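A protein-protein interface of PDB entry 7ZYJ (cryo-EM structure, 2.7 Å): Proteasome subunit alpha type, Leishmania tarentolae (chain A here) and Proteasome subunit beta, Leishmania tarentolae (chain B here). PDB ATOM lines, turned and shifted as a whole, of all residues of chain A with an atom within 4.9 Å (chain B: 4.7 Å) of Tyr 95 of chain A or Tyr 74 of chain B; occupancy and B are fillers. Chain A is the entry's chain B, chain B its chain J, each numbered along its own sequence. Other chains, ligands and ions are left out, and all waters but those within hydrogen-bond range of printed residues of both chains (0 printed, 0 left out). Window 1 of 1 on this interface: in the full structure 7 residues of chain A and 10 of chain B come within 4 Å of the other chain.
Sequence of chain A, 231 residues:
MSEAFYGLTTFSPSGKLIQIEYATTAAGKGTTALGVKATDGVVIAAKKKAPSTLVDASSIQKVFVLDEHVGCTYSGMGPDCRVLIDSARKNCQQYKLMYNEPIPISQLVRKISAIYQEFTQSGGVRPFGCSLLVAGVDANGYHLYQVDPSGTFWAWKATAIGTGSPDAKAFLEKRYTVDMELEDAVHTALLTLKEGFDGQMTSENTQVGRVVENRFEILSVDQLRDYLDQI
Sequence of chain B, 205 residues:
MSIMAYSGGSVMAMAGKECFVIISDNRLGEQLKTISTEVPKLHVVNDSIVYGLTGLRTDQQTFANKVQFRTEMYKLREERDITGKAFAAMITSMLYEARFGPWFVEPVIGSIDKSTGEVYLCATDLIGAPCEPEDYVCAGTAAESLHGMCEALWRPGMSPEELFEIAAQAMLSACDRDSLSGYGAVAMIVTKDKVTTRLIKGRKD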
ATOM      1  N   ASN A  91      14.297  19.591 -23.758  1.00  0.00           N
ATOM      2  CA  ASN A  91      13.218  19.878 -22.817  1.00  0.00           C
ATOM      3  C   ASN A  91      11.907  20.136 -23.549  1.00  0.00           C
ATOM      4  O   ASN A  91      10.843  19.676 -23.119  1.00  0.00           O
ATOM      5  CB  ASN A  91      13.589  21.074 -21.942  1.00  0.00           C
ATOM      6  CG  ASN A  91      14.511  20.697 -20.803  1.00  0.00           C
ATOM      7  OD1 ASN A  91      14.466  19.577 -20.299  1.00  0.00           O
ATOM      8  ND2 ASN A  91      15.353  21.635 -20.389  1.00  0.00           N
ATOM      9  N   CYS A  92      11.966  20.881 -24.654  1.00  0.00           N
ATOM     10  CA  CYS A  92      10.765  21.124 -25.447  1.00  0.00           C
ATOM     11  C   CYS A  92      10.192  19.820 -25.988  1.00  0.00           C
ATOM     12  O   CYS A  92       8.974  19.596 -25.944  1.00  0.00           O
ATOM     13  CB  CYS A  92      11.079  22.083 -26.594  1.00  0.00           C
ATOM     14  SG  CYS A  92      11.461  23.776 -26.099  1.00  0.00           S
ATOM     15  N   GLN A  93      11.060  18.945 -26.502  1.00  0.00           N
ATOM     16  CA  GLN A  93      10.590  17.660 -27.014  1.00  0.00           C
ATOM     17  C   GLN A  93       9.976  16.812 -25.907  1.00  0.00           C
ATOM     18  O   GLN A  93       8.936  16.174 -26.110  1.00  0.00           O
ATOM     19  CB  GLN A  93      11.735  16.913 -27.695  1.00  0.00           C
ATOM     20  CG  GLN A  93      12.082  17.442 -29.077  1.00  0.00           C
ATOM     21  CD  GLN A  93      10.887  17.485 -30.010  1.00  0.00           C
ATOM     22  OE1 GLN A  93      10.015  16.618 -29.964  1.00  0.00           O
ATOM     23  NE2 GLN A  93      10.843  18.498 -30.865  1.00  0.00           N
ATOM     24  N   GLN A  94      10.603  16.792 -24.728  1.00  0.00           N
ATOM     25  CA  GLN A  94      10.062  16.019 -23.615  1.00  0.00           C
ATOM     26  C   GLN A  94       8.710  16.561 -23.171  1.00  0.00           C
ATOM     27  O   GLN A  94       7.800  15.789 -22.846  1.00  0.00           O
ATOM     28  CB  GLN A  94      11.049  16.019 -22.449  1.00  0.00           C
ATOM     29  CG  GLN A  94      12.043  14.874 -22.483  1.00  0.00           C
ATOM     30  CD  GLN A  94      13.350  15.218 -21.798  1.00  0.00           C
ATOM     31  OE1 GLN A  94      13.419  16.154 -21.002  1.00  0.00           O
ATOM     32  NE2 GLN A  94      14.397  14.462 -22.107  1.00  0.00           N
ATOM     33  N   TYR A  95       8.561  17.887 -23.145  1.00  0.00           N
ATOM     34  CA  TYR A  95       7.277  18.477 -22.784  1.00  0.00           C
ATOM     35  C   TYR A  95       6.200  18.103 -23.795  1.00  0.00           C
ATOM     36  O   TYR A  95       5.075  17.756 -23.417  1.00  0.00           O
ATOM     37  CB  TYR A  95       7.407  19.995 -22.674  1.00  0.00           C
ATOM     38  CG  TYR A  95       6.211  20.662 -22.034  1.00  0.00           C
ATOM     39  CD1 TYR A  95       5.058  20.918 -22.763  1.00  0.00           C
ATOM     40  CD2 TYR A  95       6.236  21.034 -20.697  1.00  0.00           C
ATOM     41  CE1 TYR A  95       3.966  21.525 -22.182  1.00  0.00           C
ATOM     42  CE2 TYR A  95       5.150  21.642 -20.109  1.00  0.00           C
ATOM     43  CZ  TYR A  95       4.017  21.884 -20.855  1.00  0.00           C
ATOM     44  OH  TYR A  95       2.929  22.492 -20.273  1.00  0.00           O
ATOM     45  N   LYS A  96       6.524  18.177 -25.088  1.00  0.00           N
ATOM     46  CA  LYS A  96       5.549  17.775 -26.098  1.00  0.00           C
ATOM     47  C   LYS A  96       5.196  16.299 -25.976  1.00  0.00           C
ATOM     48  O   LYS A  96       4.052  15.911 -26.233  1.00  0.00           O
ATOM     49  CB  LYS A  96       6.070  18.084 -27.501  1.00  0.00           C
ATOM     50  CG  LYS A  96       5.813  19.509 -27.950  1.00  0.00           C
ATOM     51  CD  LYS A  96       6.250  19.726 -29.387  1.00  0.00           C
ATOM     52  CE  LYS A  96       5.959  21.146 -29.839  1.00  0.00           C
ATOM     53  NZ  LYS A  96       6.419  21.390 -31.232  1.00  0.00           N
ATOM     54  N   LEU A  97       6.162  15.463 -25.595  1.00  0.00           N
ATOM     55  CA  LEU A  97       5.871  14.049 -25.386  1.00  0.00           C
ATOM     56  C   LEU A  97       4.966  13.840 -24.178  1.00  0.00           C
ATOM     57  O   LEU A  97       4.112  12.947 -24.179  1.00  0.00           O
ATOM     58  CB  LEU A  97       7.173  13.266 -25.218  1.00  0.00           C
ATOM     59  CG  LEU A  97       7.863  12.786 -26.494  1.00  0.00           C
ATOM     60  CD1 LEU A  97       9.061  11.917 -26.153  1.00  0.00           C
ATOM     61  CD2 LEU A  97       6.890  12.034 -27.386  1.00  0.00           C
ATOM     62  N   MET A  98       5.137  14.657 -23.137  1.00  0.00           N
ATOM     63  CA  MET A  98       4.413  14.435 -21.888  1.00  0.00           C
ATOM     64  C   MET A  98       2.984  14.961 -21.943  1.00  0.00           C
ATOM     65  O   MET A  98       2.055  14.279 -21.497  1.00  0.00           O
ATOM     66  CB  MET A  98       5.168  15.082 -20.726  1.00  0.00           C
ATOM     67  CG  MET A  98       4.494  14.916 -19.372  1.00  0.00           C
ATOM     68  SD  MET A  98       4.461  13.209 -18.796  1.00  0.00           S
ATOM     69  CE  MET A  98       6.169  12.982 -18.312  1.00  0.00           C
ATOM     70  N   TYR A  99       2.781  16.163 -22.480  1.00  0.00           N
ATOM     71  CA  TYR A  99       1.488  16.830 -22.410  1.00  0.00           C
ATOM     72  C   TYR A  99       0.830  17.033 -23.767  1.00  0.00           C
ATOM     73  O   TYR A  99      -0.309  17.508 -23.817  1.00  0.00           O
ATOM     74  CB  TYR A  99       1.634  18.185 -21.707  1.00  0.00           C
ATOM     75  CG  TYR A  99       2.158  18.084 -20.293  1.00  0.00           C
ATOM     76  CD1 TYR A  99       1.362  17.586 -19.271  1.00  0.00           C
ATOM     77  CD2 TYR A  99       3.448  18.488 -19.982  1.00  0.00           C
ATOM     78  CE1 TYR A  99       1.837  17.491 -17.979  1.00  0.00           C
ATOM     79  CE2 TYR A  99       3.932  18.396 -18.692  1.00  0.00           C
ATOM     80  CZ  TYR A  99       3.122  17.898 -17.696  1.00  0.00           C
ATOM     81  OH  TYR A  99       3.599  17.806 -16.409  1.00  0.00           O
ATOM     82  N   ASN A 100       1.512  16.692 -24.862  1.00  0.00           N
ATOM     83  CA  ASN A 100       0.973  16.851 -26.214  1.00  0.00           C
ATOM     84  C   ASN A 100       0.573  18.306 -26.468  1.00  0.00           C
ATOM     85  O   ASN A 100      -0.425  18.605 -27.125  1.00  0.00           O
ATOM     86  CB  ASN A 100      -0.199  15.888 -26.448  1.00  0.00           C
ATOM     87  CG  ASN A 100      -0.736  15.938 -27.867  1.00  0.00           C
ATOM     88  OD1 ASN A 100      -1.947  15.933 -28.085  1.00  0.00           O
ATOM     89  ND2 ASN A 100       0.165  15.990 -28.839  1.00  0.00           N
ATOM     90  N   GLU A 101       1.365  19.227 -25.924  1.00  0.00           N
ATOM     91  CA  GLU A 101       1.152  20.655 -26.102  1.00  0.00           C
ATOM     92  C   GLU A 101       2.503  21.322 -26.279  1.00  0.00           C
ATOM     93  O   GLU A 101       3.514  20.801 -25.794  1.00  0.00           O
ATOM     94  CB  GLU A 101       0.417  21.276 -24.904  1.00  0.00           C
ATOM     95  CG  GLU A 101      -0.988  20.750 -24.676  1.00  0.00           C
ATOM     96  CD  GLU A 101      -1.855  21.728 -23.908  1.00  0.00           C
ATOM     97  OE1 GLU A 101      -1.296  22.564 -23.168  1.00  0.00           O
ATOM     98  OE2 GLU A 101      -3.096  21.662 -24.043  1.00  0.00           O
ATOM     99  N   PRO A 102       2.563  22.459 -26.971  1.00  0.00           N
ATOM    100  CA  PRO A 102       3.810  23.231 -27.001  1.00  0.00           C
ATOM    101  C   PRO A 102       4.156  23.736 -25.608  1.00  0.00           C
ATOM    102  O   PRO A 102       3.283  24.173 -24.856  1.00  0.00           O
ATOM    103  CB  PRO A 102       3.497  24.382 -27.964  1.00  0.00           C
ATOM    104  CG  PRO A 102       2.272  23.957 -28.707  1.00  0.00           C
ATOM    105  CD  PRO A 102       1.503  23.092 -27.769  1.00  0.00           C
ATOM    106  N   ILE A 103       5.440  23.668 -25.267  1.00  0.00           N
ATOM    107  CA  ILE A 103       5.843  24.102 -23.926  1.00  0.00           C
ATOM    108  C   ILE A 103       5.635  25.605 -23.798  1.00  0.00           C
ATOM    109  O   ILE A 103       5.983  26.362 -24.728  1.00  0.00           O
ATOM    110  CB  ILE A 103       7.302  23.708 -23.635  1.00  0.00           C
ATOM    111  CG1 ILE A 103       7.652  23.982 -22.170  1.00  0.00           C
ATOM    112  CG2 ILE A 103       8.274  24.411 -24.576  1.00  0.00           C
ATOM    113  CD1 ILE A 103       8.951  23.352 -21.725  1.00  0.00           C
ATOM    114  N   PRO A 104       5.029  26.091 -22.719  1.00  0.00           N
ATOM    115  CA  PRO A 104       4.970  27.539 -22.506  1.00  0.00           C
ATOM    116  C   PRO A 104       6.361  28.111 -22.301  1.00  0.00           C
ATOM    117  O   PRO A 104       7.263  27.447 -21.783  1.00  0.00           O
ATOM    118  CB  PRO A 104       4.108  27.689 -21.246  1.00  0.00           C
ATOM    119  CG  PRO A 104       4.056  26.339 -20.629  1.00  0.00           C
ATOM    120  CD  PRO A 104       4.262  25.340 -21.713  1.00  0.00           C
ATOM    121  N   ARG B  70       0.437  15.070  -9.400  1.00  0.00           N
ATOM    122  CA  ARG B  70       0.893  15.622 -10.671  1.00  0.00           C
ATOM    123  C   ARG B  70       0.161  16.911 -11.019  1.00  0.00           C
ATOM    124  O   ARG B  70       0.782  17.874 -11.477  1.00  0.00           O
ATOM    125  CB  ARG B  70       0.720  14.584 -11.779  1.00  0.00           C
ATOM    126  CG  ARG B  70       1.794  13.515 -11.781  1.00  0.00           C
ATOM    127  CD  ARG B  70       3.137  14.095 -12.183  1.00  0.00           C
ATOM    128  NE  ARG B  70       3.339  14.068 -13.626  1.00  0.00           N
ATOM    129  CZ  ARG B  70       3.602  12.974 -14.327  1.00  0.00           C
ATOM    130  NH1 ARG B  70       3.727  11.792 -13.745  1.00  0.00           N
ATOM    131  NH2 ARG B  70       3.746  13.068 -15.646  1.00  0.00           N
ATOM    132  N   THR B  71      -1.155  16.957 -10.803  1.00  0.00           N
ATOM    133  CA  THR B  71      -1.915  18.156 -11.141  1.00  0.00           C
ATOM    134  C   THR B  71      -1.579  19.314 -10.211  1.00  0.00           C
ATOM    135  O   THR B  71      -1.504  20.466 -10.654  1.00  0.00           O
ATOM    136  CB  THR B  71      -3.418  17.869 -11.112  1.00  0.00           C
ATOM    137  OG1 THR B  71      -3.802  17.423  -9.806  1.00  0.00           O
ATOM    138  CG2 THR B  71      -3.787  16.821 -12.149  1.00  0.00           C
ATOM    139  N   GLU B  72      -1.373  19.040  -8.920  1.00  0.00           N
ATOM    140  CA  GLU B  72      -0.962  20.109  -8.016  1.00  0.00           C
ATOM    141  C   GLU B  72       0.418  20.643  -8.382  1.00  0.00           C
ATOM    142  O   GLU B  72       0.640  21.860  -8.367  1.00  0.00           O
ATOM    143  CB  GLU B  72      -0.987  19.625  -6.566  1.00  0.00           C
ATOM    144  CG  GLU B  72      -2.359  19.203  -6.070  1.00  0.00           C
ATOM    145  CD  GLU B  72      -3.420  20.260  -6.305  1.00  0.00           C
ATOM    146  OE1 GLU B  72      -3.136  21.456  -6.090  1.00  0.00           O
ATOM    147  OE2 GLU B  72      -4.543  19.891  -6.710  1.00  0.00           O
ATOM    148  N   MET B  73       1.354  19.753  -8.722  1.00  0.00           N
ATOM    149  CA  MET B  73       2.671  20.211  -9.153  1.00  0.00           C
ATOM    150  C   MET B  73       2.577  21.017 -10.442  1.00  0.00           C
ATOM    151  O   MET B  73       3.276  22.024 -10.607  1.00  0.00           O
ATOM    152  CB  MET B  73       3.611  19.020  -9.330  1.00  0.00           C
ATOM    153  CG  MET B  73       5.084  19.386  -9.303  1.00  0.00           C
ATOM    154  SD  MET B  73       5.605  20.099  -7.730  1.00  0.00           S
ATOM    155  CE  MET B  73       5.868  21.808  -8.194  1.00  0.00           C
ATOM    156  N   TYR B  74       1.722  20.584 -11.369  1.00  0.00           N
ATOM    157  CA  TYR B  74       1.533  21.307 -12.621  1.00  0.00           C
ATOM    158  C   TYR B  74       0.983  22.704 -12.367  1.00  0.00           C
ATOM    159  O   TYR B  74       1.448  23.686 -12.956  1.00  0.00           O
ATOM    160  CB  TYR B  74       0.602  20.506 -13.535  1.00  0.00           C
ATOM    161  CG  TYR B  74       0.330  21.114 -14.895  1.00  0.00           C
ATOM    162  CD1 TYR B  74      -0.615  22.118 -15.058  1.00  0.00           C
ATOM    163  CD2 TYR B  74       1.003  20.664 -16.021  1.00  0.00           C
ATOM    164  CE1 TYR B  74      -0.869  22.666 -16.297  1.00  0.00           C
ATOM    165  CE2 TYR B  74       0.754  21.205 -17.265  1.00  0.00           C
ATOM    166  CZ  TYR B  74      -0.183  22.204 -17.397  1.00  0.00           C
ATOM    167  OH  TYR B  74      -0.433  22.746 -18.634  1.00  0.00           O
ATOM    168  N   LYS B  75      -0.014  22.814 -11.487  1.00  0.00           N
ATOM    169  CA  LYS B  75      -0.596  24.117 -11.195  1.00  0.00           C
ATOM    170  C   LYS B  75       0.370  25.004 -10.421  1.00  0.00           C
ATOM    171  O   LYS B  75       0.293  26.234 -10.519  1.00  0.00           O
ATOM    172  CB  LYS B  75      -1.904  23.952 -10.424  1.00  0.00           C
ATOM    173  CG  LYS B  75      -2.793  25.182 -10.458  1.00  0.00           C
ATOM    174  CD  LYS B  75      -4.155  24.898  -9.856  1.00  0.00           C
ATOM    175  CE  LYS B  75      -4.893  26.188  -9.540  1.00  0.00           C
ATOM    176  NZ  LYS B  75      -4.945  27.102 -10.714  1.00  0.00           N
ATOM    177  N   LEU B  76       1.276  24.408  -9.645  1.00  0.00           N
ATOM    178  CA  LEU B  76       2.291  25.204  -8.961  1.00  0.00           C
ATOM    179  C   LEU B  76       3.344  25.705  -9.941  1.00  0.00           C
ATOM    180  O   LEU B  76       3.640  26.904  -9.991  1.00  0.00           O
ATOM    181  CB  LEU B  76       2.935  24.384  -7.845  1.00  0.00           C
ATOM    182  CG  LEU B  76       2.163  24.321  -6.528  1.00  0.00           C
ATOM    183  CD1 LEU B  76       2.855  23.387  -5.553  1.00  0.00           C
ATOM    184  CD2 LEU B  76       2.010  25.709  -5.931  1.00  0.00           C
ATOM    185  N   ARG B  77       3.925  24.796 -10.728  1.00  0.00           N
ATOM    186  CA  ARG B  77       4.914  25.190 -11.727  1.00  0.00           C
ATOM    187  C   ARG B  77       4.291  26.090 -12.786  1.00  0.00           C
ATOM    188  O   ARG B  77       4.690  27.248 -12.952  1.00  0.00           O
ATOM    189  CB  ARG B  77       5.529  23.946 -12.369  1.00  0.00           C
ATOM    190  CG  ARG B  77       6.546  23.239 -11.499  1.00  0.00           C
ATOM    191  CD  ARG B  77       7.597  22.541 -12.341  1.00  0.00           C
ATOM    192  NE  ARG B  77       8.010  21.273 -11.752  1.00  0.00           N
ATOM    193  CZ  ARG B  77       7.341  20.136 -11.875  1.00  0.00           C
ATOM    194  NH1 ARG B  77       6.214  20.067 -12.565  1.00  0.00           N
ATOM    195  NH2 ARG B  77       7.812  19.039 -11.288  1.00  0.00           N
ATOM    196  N   GLU B  78       3.309  25.570 -13.516  1.00  0.00           N
ATOM    197  CA  GLU B  78       2.596  26.355 -14.515  1.00  0.00           C
ATOM    198  C   GLU B  78       1.452  27.085 -13.829  1.00  0.00           C
ATOM    199  O   GLU B  78       0.524  26.455 -13.313  1.00  0.00           O
ATOM    200  CB  GLU B  78       2.077  25.462 -15.636  1.00  0.00           C
ATOM    201  CG  GLU B  78       3.090  24.462 -16.145  1.00  0.00           C
ATOM    202  CD  GLU B  78       2.750  23.953 -17.525  1.00  0.00           C
ATOM    203  OE1 GLU B  78       1.785  24.466 -18.129  1.00  0.00           O
ATOM    204  OE2 GLU B  78       3.445  23.035 -18.006  1.00  0.00           O
ATOM    205  N   ARG B  80      -1.474  28.047 -14.050  1.00  0.00           N
ATOM    206  CA  ARG B  80      -2.702  27.886 -14.819  1.00  0.00           C
ATOM    207  C   ARG B  80      -3.271  26.506 -14.530  1.00  0.00           C
ATOM    208  O   ARG B  80      -2.558  25.604 -14.083  1.00  0.00           O
ATOM    209  CB  ARG B  80      -2.462  28.054 -16.324  1.00  0.00           C
ATOM    210  CG  ARG B  80      -1.431  27.101 -16.896  1.00  0.00           C
ATOM    211  CD  ARG B  80      -1.534  27.021 -18.407  1.00  0.00           C
ATOM    212  NE  ARG B  80      -0.523  26.138 -18.972  1.00  0.00           N
ATOM    213  CZ  ARG B  80      -0.544  25.672 -20.213  1.00  0.00           C
ATOM    214  NH1 ARG B  80      -1.517  25.986 -21.051  1.00  0.00           N
ATOM    215  NH2 ARG B  80       0.435  24.870 -20.622  1.00  0.00           N
ATOM    216  N   ASP B  81      -4.566  26.357 -14.788  1.00  0.00           N
ATOM    217  CA  ASP B  81      -5.224  25.064 -14.701  1.00  0.00           C
ATOM    218  C   ASP B  81      -4.856  24.217 -15.910  1.00  0.00           C
ATOM    219  O   ASP B  81      -4.767  24.721 -17.034  1.00  0.00           O
ATOM    220  CB  ASP B  81      -6.742  25.227 -14.623  1.00  0.00           C
ATOM    221  CG  ASP B  81      -7.218  25.611 -13.237  1.00  0.00           C
ATOM    222  OD1 ASP B  81      -6.588  25.178 -12.251  1.00  0.00           O
ATOM    223  OD2 ASP B  81      -8.225  26.342 -13.134  1.00  0.00           O
ATOM    224  N   ILE B  82      -4.637  22.924 -15.672  1.00  0.00           N
ATOM    225  CA  ILE B  82      -4.343  22.011 -16.766  1.00  0.00           C
ATOM    226  C   ILE B  82      -5.577  21.854 -17.647  1.00  0.00           C
ATOM    227  O   ILE B  82      -6.722  21.924 -17.180  1.00  0.00           O
ATOM    228  CB  ILE B  82      -3.852  20.654 -16.225  1.00  0.00           C
ATOM    229  CG1 ILE B  82      -3.144  19.859 -17.323  1.00  0.00           C
ATOM    230  CG2 ILE B  82      -4.999  19.857 -15.620  1.00  0.00           C
ATOM    231  CD1 ILE B  82      -2.331  18.699 -16.804  1.00  0.00           C
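NH2 of Arg 70 of chain B is in hydrogen-bond range of SD of Met 98 of chain A (3.2 Å).
OE1 of Glu 78 of chain B lies close to OH of Tyr 95 of chain A, at 3.1 Å.
The guanidinium group of Arg 80 of chain B sits at hydrogen-bond distance from the side-chain hydroxyl of Tyr 95 of chain A (3.5 Å).
The guanidinium group of Arg 80 of chain B is in salt-bridge range of the side-chain carboxylate of Glu 101 of chain A, 3.8 Å away.
The side-chain hydroxyl (OH) of Tyr 74 of chain B is in hydrogen-bond range of the side-chain carboxylate (OE1) of Glu 78 of chain B (2.9 Å).
The side-chain hydroxyl (OH) of Tyr 74 of chain B sits at hydrogen-bond distance from the guanidinium group (NH2) of Arg 80 of chain B, 3.0 Å away.
OE1 of Glu 78 of chain B lies within salt-bridge range of NH2 of Arg 80 of chain B (2.9 Å).
Among the printed residues, pairs that only touch across the chains: Tyr 95 of chain A with Tyr 74 of chain B (3.7 Å), Tyr 99 of chain A with Tyr 74 of chain B (3.8 Å), Pro 104 of chain A with Glu 78 of chain B (3.9 Å) and Pro 104 of chain A with Arg 80 of chain B (3.9 Å).
Gln 94 of chain A touches none of the printed residues of chain B.
Tyr 95 of chain A touches just these residues of chain B: Tyr 74, Glu 78 and Arg 80.
Of the printed residues of chain B, Met 98 of chain A touches Arg 70 (3.2 Å).
Of the printed residues of chain B, Tyr 99 of chain A touches Tyr 74 (3.8 Å).
Printed residues of chain B within 4 Å of Glu 101 of chain A: Arg 80 (3.8 Å).
Tyr 74 of chain B touches just these residues of chain A: Tyr 95 (3.7 Å) and Tyr 99 (3.8 Å).
Of the printed residues of chain A, Glu 78 of chain B touches Tyr 95 (2.4 Å) and Pro 104 (3.9 Å).
Printed residues of chain A that touch a printed residue of chain B: Tyr 95, Met 98, Tyr 99, Glu 101 and Pro 104.
Hydrophobic or aromatic side chains of chain A that line the printed part of chain B: Tyr 95, Met 98, Tyr 99 and Pro 104.
Hydrophobic or aromatic side chains of chain B that line the printed part of chain A: Tyr 74.
Among the printed residues, 8 pairs touch across the chains.
Among the printed residues, Asp or Glu carboxylates within 4 Å of a Lys or Arg side-chain nitrogen of the other chain: Glu 101 of chain A with Arg 80 of chain B (3.8 Å).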
